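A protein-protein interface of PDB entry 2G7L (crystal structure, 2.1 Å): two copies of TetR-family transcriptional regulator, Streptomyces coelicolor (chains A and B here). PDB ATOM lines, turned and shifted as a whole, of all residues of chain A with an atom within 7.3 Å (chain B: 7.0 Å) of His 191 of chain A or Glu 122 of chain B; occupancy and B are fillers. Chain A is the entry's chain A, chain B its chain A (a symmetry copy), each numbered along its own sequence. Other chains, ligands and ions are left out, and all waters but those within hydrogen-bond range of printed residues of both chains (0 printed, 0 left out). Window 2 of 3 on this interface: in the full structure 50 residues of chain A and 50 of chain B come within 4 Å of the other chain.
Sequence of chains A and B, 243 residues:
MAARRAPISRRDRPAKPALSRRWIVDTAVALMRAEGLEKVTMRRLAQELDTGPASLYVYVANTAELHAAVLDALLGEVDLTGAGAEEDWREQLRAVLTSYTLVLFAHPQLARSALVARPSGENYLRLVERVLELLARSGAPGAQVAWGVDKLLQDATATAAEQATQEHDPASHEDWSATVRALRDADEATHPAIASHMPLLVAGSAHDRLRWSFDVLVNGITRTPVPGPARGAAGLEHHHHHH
The side-chain carboxylate (OE2) of Glu 122 of chain B lies within hydrogen-bond range of a ring nitrogen (NE2) of His 191 of chain A.
The side-chain carboxylate of Glu 129 of chain B is in hydrogen-bond range of the backbone NH of Ala 193 of chain A (2.7 Å).
The backbone NH (N) of Ile 194 of chain A is in hydrogen-bond range of the side-chain carboxylate (OE1) of Glu 129 of chain B.
The backbone nitrogen of Pro 192 of chain A lies close to the side-chain carboxylate of Glu 129 of chain B, 3.2 Å away.
O of Ala 193 of chain A is in hydrogen-bond range of ND1 of His 197 of chain A, at 2.8 Å.
Among the printed residues, pairs that only touch across the chains: Ala 182 of chain A with Ser 120 of chain B (3.7 Å), Ala 182 of chain A with Leu 125 of chain B (3.5 Å), His 191 of chain A with Leu 125 of chain B (3.7 Å), His 191 of chain A with Glu 129 of chain B (3.3 Å) and Ile 194 of chain A with Leu 125 of chain B (3.4 Å).
Of the printed residues of chain B, His 191 of chain A touches Glu 122, Leu 125 and Glu 129.
Printed residues of chain A within 4 Å of Glu 122 of chain B: His 191 (2.8 Å).
Printed residues of chain A within 4 Å of Glu 129 of chain B: His 191 (3.3 Å), Pro 192 (3.0 Å), Ala 193 (2.7 Å) and Ile 194 (2.9 Å).
Printed residues of chain A within 4 Å of Leu 125 of chain B: Ala 182 (3.5 Å), His 191 (3.7 Å) and Ile 194 (3.4 Å).
Val 128 of chain B touches none of the printed residues of chain A.
The nearest printed residue of chain A that does not touch Glu 122 of chain B is Thr 190 of chain A (6.4 Å).
The nearest printed residue of chain B that does not touch Ala 182 of chain A is Gly 121 of chain B (5.7 Å).
Hydrophobic or aromatic side chains of chain A within 4 Å of the printed part of chain B: Ala 182, His 191, Pro 192, Ala 193 and Ile 194.
Among the printed residues, no Asp or Glu carboxylate lies within 4 Å of a Lys or Arg side-chain nitrogen of the other chain.
No position is printed for both chains.
Of the 9 pairs that touch across the chains among the printed residues, none has its exchanged pair printed and touching as well.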
ATOM      1  N   ALA A 182     -20.054  18.682  11.125  1.00  0.00           N
ATOM      2  CA  ALA A 182     -20.512  19.038  12.460  1.00  0.00           C
ATOM      3  C   ALA A 182     -20.777  20.544  12.605  1.00  0.00           C
ATOM      4  O   ALA A 182     -21.677  20.957  13.364  1.00  0.00           O
ATOM      5  CB  ALA A 182     -19.528  18.544  13.513  1.00  0.00           C
ATOM      6  N   LEU A 183     -19.989  21.350  11.887  1.00  0.00           N
ATOM      7  CA  LEU A 183     -20.133  22.802  11.878  1.00  0.00           C
ATOM      8  C   LEU A 183     -21.389  23.190  11.084  1.00  0.00           C
ATOM      9  O   LEU A 183     -22.191  23.989  11.583  1.00  0.00           O
ATOM     10  CB  LEU A 183     -18.892  23.505  11.314  1.00  0.00           C
ATOM     11  CG  LEU A 183     -17.725  24.091  12.156  1.00  0.00           C
ATOM     12  CD1 LEU A 183     -17.888  24.193  13.727  1.00  0.00           C
ATOM     13  CD2 LEU A 183     -16.348  23.624  11.758  1.00  0.00           C
ATOM     14  N   ASP A 185     -24.009  21.467  10.855  1.00  0.00           N
ATOM     15  CA  ASP A 185     -25.134  20.882  11.607  1.00  0.00           C
ATOM     16  C   ASP A 185     -25.344  21.475  12.989  1.00  0.00           C
ATOM     17  O   ASP A 185     -26.405  21.224  13.601  1.00  0.00           O
ATOM     18  CB  ASP A 185     -24.927  19.379  11.869  1.00  0.00           C
ATOM     19  CG  ASP A 185     -25.039  18.544  10.630  1.00  0.00           C
ATOM     20  OD1 ASP A 185     -25.843  18.892   9.726  1.00  0.00           O
ATOM     21  OD2 ASP A 185     -24.329  17.513  10.571  1.00  0.00           O
ATOM     22  N   ALA A 186     -24.320  22.169  13.517  1.00  0.00           N
ATOM     23  CA  ALA A 186     -24.463  22.928  14.764  1.00  0.00           C
ATOM     24  C   ALA A 186     -25.757  23.741  14.677  1.00  0.00           C
ATOM     25  O   ALA A 186     -26.087  24.305  13.625  1.00  0.00           O
ATOM     26  CB  ALA A 186     -23.260  23.844  15.022  1.00  0.00           C
ATOM     27  N   ASP A 187     -26.494  23.761  15.783  1.00  0.00           N
ATOM     28  CA  ASP A 187     -27.792  24.429  15.840  1.00  0.00           C
ATOM     29  C   ASP A 187     -27.603  25.891  16.175  1.00  0.00           C
ATOM     30  O   ASP A 187     -27.020  26.213  17.209  1.00  0.00           O
ATOM     31  CB  ASP A 187     -28.746  23.739  16.857  1.00  0.00           C
ATOM     32  CG  ASP A 187     -29.234  22.345  16.378  1.00  0.00           C
ATOM     33  OD1 ASP A 187     -29.828  22.230  15.268  1.00  0.00           O
ATOM     34  OD2 ASP A 187     -29.027  21.355  17.121  1.00  0.00           O
ATOM     35  N   GLU A 188     -28.109  26.754  15.285  1.00  0.00           N
ATOM     36  CA  GLU A 188     -28.205  28.206  15.498  1.00  0.00           C
ATOM     37  C   GLU A 188     -28.543  28.568  16.946  1.00  0.00           C
ATOM     38  O   GLU A 188     -27.974  29.495  17.517  1.00  0.00           O
ATOM     39  CB  GLU A 188     -29.161  28.837  14.450  1.00  0.00           C
ATOM     40  CG  GLU A 188     -30.210  29.891  14.947  1.00  0.00           C
ATOM     41  CD  GLU A 188     -29.718  31.350  14.990  1.00  0.00           C
ATOM     42  OE1 GLU A 188     -29.022  31.730  15.967  1.00  0.00           O
ATOM     43  OE2 GLU A 188     -30.068  32.134  14.068  1.00  0.00           O
ATOM     44  N   ALA A 189     -29.421  27.776  17.553  1.00  0.00           N
ATOM     45  CA  ALA A 189     -29.893  27.991  18.921  1.00  0.00           C
ATOM     46  C   ALA A 189     -28.777  27.855  19.961  1.00  0.00           C
ATOM     47  O   ALA A 189     -28.591  28.741  20.831  1.00  0.00           O
ATOM     48  CB  ALA A 189     -31.028  27.002  19.223  1.00  0.00           C
ATOM     49  N   THR A 190     -28.034  26.754  19.828  1.00  0.00           N
ATOM     50  CA  THR A 190     -26.984  26.260  20.777  1.00  0.00           C
ATOM     51  C   THR A 190     -25.540  26.764  20.485  1.00  0.00           C
ATOM     52  O   THR A 190     -24.664  26.774  21.365  1.00  0.00           O
ATOM     53  CB  THR A 190     -26.945  24.722  20.660  1.00  0.00           C
ATOM     54  OG1 THR A 190     -27.257  24.361  19.298  1.00  0.00           O
ATOM     55  CG2 THR A 190     -28.000  24.081  21.560  1.00  0.00           C
ATOM     56  N   HIS A 191     -25.318  27.152  19.235  1.00  0.00           N
ATOM     57  CA  HIS A 191     -24.018  27.601  18.735  1.00  0.00           C
ATOM     58  C   HIS A 191     -24.230  28.798  17.798  1.00  0.00           C
ATOM     59  O   HIS A 191     -24.028  28.672  16.585  1.00  0.00           O
ATOM     60  CB  HIS A 191     -23.358  26.468  17.942  1.00  0.00           C
ATOM     61  CG  HIS A 191     -22.940  25.304  18.779  1.00  0.00           C
ATOM     62  ND1 HIS A 191     -23.653  24.136  18.823  1.00  0.00           N
ATOM     63  CD2 HIS A 191     -21.866  25.121  19.592  1.00  0.00           C
ATOM     64  CE1 HIS A 191     -23.052  23.285  19.643  1.00  0.00           C
ATOM     65  NE2 HIS A 191     -21.960  23.854  20.121  1.00  0.00           N
ATOM     66  N   PRO A 192     -24.701  29.950  18.346  1.00  0.00           N
ATOM     67  CA  PRO A 192     -25.044  31.076  17.480  1.00  0.00           C
ATOM     68  C   PRO A 192     -23.780  31.723  16.805  1.00  0.00           C
ATOM     69  O   PRO A 192     -23.842  32.129  15.657  1.00  0.00           O
ATOM     70  CB  PRO A 192     -25.724  32.045  18.448  1.00  0.00           C
ATOM     71  CG  PRO A 192     -25.021  31.752  19.781  1.00  0.00           C
ATOM     72  CD  PRO A 192     -24.915  30.272  19.773  1.00  0.00           C
ATOM     73  N   ALA A 193     -22.655  31.767  17.506  1.00  0.00           N
ATOM     74  CA  ALA A 193     -21.411  32.325  16.910  1.00  0.00           C
ATOM     75  C   ALA A 193     -21.035  31.474  15.702  1.00  0.00           C
ATOM     76  O   ALA A 193     -20.743  32.032  14.651  1.00  0.00           O
ATOM     77  CB  ALA A 193     -20.275  32.409  17.932  1.00  0.00           C
ATOM     78  N   ILE A 194     -21.149  30.143  15.792  1.00  0.00           N
ATOM     79  CA  ILE A 194     -20.884  29.278  14.608  1.00  0.00           C
ATOM     80  C   ILE A 194     -21.846  29.562  13.470  1.00  0.00           C
ATOM     81  O   ILE A 194     -21.428  29.744  12.315  1.00  0.00           O
ATOM     82  CB  ILE A 194     -20.836  27.789  14.940  1.00  0.00           C
ATOM     83  CG1 ILE A 194     -19.641  27.501  15.881  1.00  0.00           C
ATOM     84  CG2 ILE A 194     -20.723  26.967  13.651  1.00  0.00           C
ATOM     85  CD1 ILE A 194     -19.620  26.069  16.584  1.00  0.00           C
ATOM     86  N   ALA A 195     -23.136  29.645  13.772  1.00  0.00           N
ATOM     87  CA  ALA A 195     -24.096  29.879  12.701  1.00  0.00           C
ATOM     88  C   ALA A 195     -23.831  31.218  12.044  1.00  0.00           C
ATOM     89  O   ALA A 195     -23.882  31.335  10.811  1.00  0.00           O
ATOM     90  CB  ALA A 195     -25.586  29.821  13.238  1.00  0.00           C
ATOM     91  N   SER A 196     -23.603  32.222  12.885  1.00  0.00           N
ATOM     92  CA  SER A 196     -23.264  33.589  12.460  1.00  0.00           C
ATOM     93  C   SER A 196     -22.105  33.641  11.405  1.00  0.00           C
ATOM     94  O   SER A 196     -22.081  34.472  10.456  1.00  0.00           O
ATOM     95  CB  SER A 196     -22.912  34.342  13.745  1.00  0.00           C
ATOM     96  OG  SER A 196     -22.571  35.676  13.491  1.00  0.00           O
ATOM     97  N   HIS A 197     -21.167  32.706  11.544  1.00  0.00           N
ATOM     98  CA  HIS A 197     -19.932  32.713  10.730  1.00  0.00           C
ATOM     99  C   HIS A 197     -19.846  31.664   9.613  1.00  0.00           C
ATOM    100  O   HIS A 197     -18.820  31.540   8.951  1.00  0.00           O
ATOM    101  CB  HIS A 197     -18.743  32.680  11.641  1.00  0.00           C
ATOM    102  CG  HIS A 197     -18.602  33.936  12.457  1.00  0.00           C
ATOM    103  ND1 HIS A 197     -19.056  34.040  13.753  1.00  0.00           N
ATOM    104  CD2 HIS A 197     -18.046  35.135  12.159  1.00  0.00           C
ATOM    105  CE1 HIS A 197     -18.772  35.237  14.230  1.00  0.00           C
ATOM    106  NE2 HIS A 197     -18.158  35.924  13.280  1.00  0.00           N
ATOM    107  N   ASP B  72     -11.033  15.254  21.471  1.00  0.00           N
ATOM    108  CA  ASP B  72     -12.291  15.911  21.841  1.00  0.00           C
ATOM    109  C   ASP B  72     -12.707  15.682  23.298  1.00  0.00           C
ATOM    110  O   ASP B  72     -12.951  16.627  24.054  1.00  0.00           O
ATOM    111  CB  ASP B  72     -13.416  15.583  20.885  1.00  0.00           C
ATOM    112  CG  ASP B  72     -14.602  16.534  21.050  1.00  0.00           C
ATOM    113  OD1 ASP B  72     -15.269  16.430  22.089  1.00  0.00           O
ATOM    114  OD2 ASP B  72     -14.913  17.359  20.156  1.00  0.00           O
ATOM    115  N   LEU B  80     -14.138  27.389  29.233  1.00  0.00           N
ATOM    116  CA  LEU B  80     -14.830  28.251  28.281  1.00  0.00           C
ATOM    117  C   LEU B  80     -15.728  29.280  29.010  1.00  0.00           C
ATOM    118  O   LEU B  80     -16.714  29.809  28.462  1.00  0.00           O
ATOM    119  CB  LEU B  80     -15.653  27.388  27.324  1.00  0.00           C
ATOM    120  CG  LEU B  80     -14.892  26.334  26.508  1.00  0.00           C
ATOM    121  CD1 LEU B  80     -15.806  25.841  25.461  1.00  0.00           C
ATOM    122  CD2 LEU B  80     -13.637  26.898  25.876  1.00  0.00           C
ATOM    123  N   SER B 120     -14.281  16.845  16.073  1.00  0.00           N
ATOM    124  CA  SER B 120     -15.575  17.221  15.576  1.00  0.00           C
ATOM    125  C   SER B 120     -16.653  16.951  16.639  1.00  0.00           C
ATOM    126  O   SER B 120     -17.822  16.932  16.325  1.00  0.00           O
ATOM    127  CB  SER B 120     -15.886  16.459  14.291  1.00  0.00           C
ATOM    128  OG  SER B 120     -15.945  15.053  14.530  1.00  0.00           O
ATOM    129  N   GLY B 121     -16.284  16.757  17.894  1.00  0.00           N
ATOM    130  CA  GLY B 121     -17.314  16.418  18.855  1.00  0.00           C
ATOM    131  C   GLY B 121     -17.810  17.645  19.558  1.00  0.00           C
ATOM    132  O   GLY B 121     -17.451  18.775  19.192  1.00  0.00           O
ATOM    133  N   GLU B 122     -18.609  17.443  20.609  1.00  0.00           N
ATOM    134  CA  GLU B 122     -19.246  18.580  21.279  1.00  0.00           C
ATOM    135  C   GLU B 122     -18.295  19.582  21.923  1.00  0.00           C
ATOM    136  O   GLU B 122     -18.560  20.792  21.913  1.00  0.00           O
ATOM    137  CB  GLU B 122     -20.317  18.151  22.320  1.00  0.00           C
ATOM    138  CG  GLU B 122     -21.282  19.332  22.666  1.00  0.00           C
ATOM    139  CD  GLU B 122     -21.640  20.225  21.426  1.00  0.00           C
ATOM    140  OE1 GLU B 122     -22.379  19.747  20.521  1.00  0.00           O
ATOM    141  OE2 GLU B 122     -21.197  21.410  21.365  1.00  0.00           O
ATOM    142  N   ASN B 123     -17.225  19.072  22.511  1.00  0.00           N
ATOM    143  CA  ASN B 123     -16.288  19.896  23.229  1.00  0.00           C
ATOM    144  C   ASN B 123     -15.496  20.824  22.273  1.00  0.00           C
ATOM    145  O   ASN B 123     -15.142  21.953  22.647  1.00  0.00           O
ATOM    146  CB  ASN B 123     -15.347  19.022  24.035  1.00  0.00           C
ATOM    147  CG  ASN B 123     -16.066  18.300  25.217  1.00  0.00           C
ATOM    148  OD1 ASN B 123     -16.909  18.894  25.883  1.00  0.00           O
ATOM    149  ND2 ASN B 123     -15.672  17.059  25.504  1.00  0.00           N
ATOM    150  N   TYR B 124     -15.251  20.347  21.049  1.00  0.00           N
ATOM    151  CA  TYR B 124     -14.465  21.084  20.072  1.00  0.00           C
ATOM    152  C   TYR B 124     -15.375  22.130  19.484  1.00  0.00           C
ATOM    153  O   TYR B 124     -14.980  23.293  19.379  1.00  0.00           O
ATOM    154  CB  TYR B 124     -13.871  20.193  18.953  1.00  0.00           C
ATOM    155  CG  TYR B 124     -12.860  20.940  18.046  1.00  0.00           C
ATOM    156  CD1 TYR B 124     -11.601  21.284  18.523  1.00  0.00           C
ATOM    157  CD2 TYR B 124     -13.168  21.281  16.750  1.00  0.00           C
ATOM    158  CE1 TYR B 124     -10.646  21.968  17.704  1.00  0.00           C
ATOM    159  CE2 TYR B 124     -12.222  21.962  15.913  1.00  0.00           C
ATOM    160  CZ  TYR B 124     -10.965  22.301  16.421  1.00  0.00           C
ATOM    161  OH  TYR B 124      -9.982  22.968  15.644  1.00  0.00           O
ATOM    162  N   LEU B 125     -16.584  21.728  19.102  1.00  0.00           N
ATOM    163  CA  LEU B 125     -17.602  22.694  18.688  1.00  0.00           C
ATOM    164  C   LEU B 125     -17.858  23.797  19.750  1.00  0.00           C
ATOM    165  O   LEU B 125     -18.129  24.938  19.388  1.00  0.00           O
ATOM    166  CB  LEU B 125     -18.914  21.961  18.322  1.00  0.00           C
ATOM    167  CG  LEU B 125     -19.103  21.711  16.820  1.00  0.00           C
ATOM    168  CD1 LEU B 125     -17.882  20.991  16.232  1.00  0.00           C
ATOM    169  CD2 LEU B 125     -20.371  20.888  16.641  1.00  0.00           C
ATOM    170  N   ARG B 126     -17.760  23.455  21.034  1.00  0.00           N
ATOM    171  CA  ARG B 126     -17.854  24.444  22.098  1.00  0.00           C
ATOM    172  C   ARG B 126     -16.639  25.369  22.222  1.00  0.00           C
ATOM    173  O   ARG B 126     -16.786  26.576  22.488  1.00  0.00           O
ATOM    174  CB  ARG B 126     -18.134  23.797  23.473  1.00  0.00           C
ATOM    175  CG  ARG B 126     -19.662  23.445  23.676  1.00  0.00           C
ATOM    176  CD  ARG B 126     -19.909  22.868  25.090  1.00  0.00           C
ATOM    177  NE  ARG B 126     -18.691  22.284  25.664  1.00  0.00           N
ATOM    178  CZ  ARG B 126     -18.040  22.739  26.743  1.00  0.00           C
ATOM    179  NH1 ARG B 126     -18.501  23.814  27.401  1.00  0.00           N
ATOM    180  NH2 ARG B 126     -16.916  22.115  27.158  1.00  0.00           N
ATOM    181  N   LEU B 127     -15.442  24.778  22.126  1.00  0.00           N
ATOM    182  CA  LEU B 127     -14.218  25.563  21.946  1.00  0.00           C
ATOM    183  C   LEU B 127     -14.335  26.488  20.777  1.00  0.00           C
ATOM    184  O   LEU B 127     -14.098  27.657  20.943  1.00  0.00           O
ATOM    185  CB  LEU B 127     -12.993  24.677  21.758  1.00  0.00           C
ATOM    186  CG  LEU B 127     -11.653  25.418  21.556  1.00  0.00           C
ATOM    187  CD1 LEU B 127     -11.105  25.915  22.900  1.00  0.00           C
ATOM    188  CD2 LEU B 127     -10.695  24.359  20.971  1.00  0.00           C
ATOM    189  N   VAL B 128     -14.691  26.006  19.599  1.00  0.00           N
ATOM    190  CA  VAL B 128     -14.777  26.913  18.469  1.00  0.00           C
ATOM    191  C   VAL B 128     -15.807  28.029  18.634  1.00  0.00           C
ATOM    192  O   VAL B 128     -15.501  29.178  18.317  1.00  0.00           O
ATOM    193  CB  VAL B 128     -14.637  26.292  16.967  1.00  0.00           C
ATOM    194  CG1 VAL B 128     -14.154  24.826  16.882  1.00  0.00           C
ATOM    195  CG2 VAL B 128     -15.663  26.798  15.890  1.00  0.00           C
ATOM    196  N   GLU B 129     -16.995  27.689  19.177  1.00  0.00           N
ATOM    197  CA  GLU B 129     -18.078  28.672  19.391  1.00  0.00           C
ATOM    198  C   GLU B 129     -17.538  29.824  20.260  1.00  0.00           C
ATOM    199  O   GLU B 129     -17.722  30.963  19.964  1.00  0.00           O
ATOM    200  CB  GLU B 129     -19.288  27.953  20.084  1.00  0.00           C
ATOM    201  CG  GLU B 129     -20.317  28.900  20.651  1.00  0.00           C
ATOM    202  CD  GLU B 129     -21.141  29.486  19.563  1.00  0.00           C
ATOM    203  OE1 GLU B 129     -21.031  28.935  18.441  1.00  0.00           O
ATOM    204  OE2 GLU B 129     -21.879  30.509  19.814  1.00  0.00           O
ATOM    205  N   ARG B 130     -16.861  29.486  21.333  1.00  0.00           N
ATOM    206  CA  ARG B 130     -16.333  30.416  22.262  1.00  0.00           C
ATOM    207  C   ARG B 130     -15.175  31.279  21.693  1.00  0.00           C
ATOM    208  O   ARG B 130     -15.024  32.445  22.040  1.00  0.00           O
ATOM    209  CB  ARG B 130     -15.786  29.606  23.432  1.00  0.00           C
ATOM    210  CG  ARG B 130     -15.147  30.458  24.566  1.00  0.00           C
ATOM    211  CD  ARG B 130     -16.212  31.454  25.184  1.00  0.00           C
ATOM    212  NE  ARG B 130     -15.648  32.129  26.357  1.00  0.00           N
ATOM    213  CZ  ARG B 130     -16.087  33.296  26.839  1.00  0.00           C
ATOM    214  NH1 ARG B 130     -17.097  33.956  26.234  1.00  0.00           N
ATOM    215  NH2 ARG B 130     -15.470  33.806  27.896  1.00  0.00           N
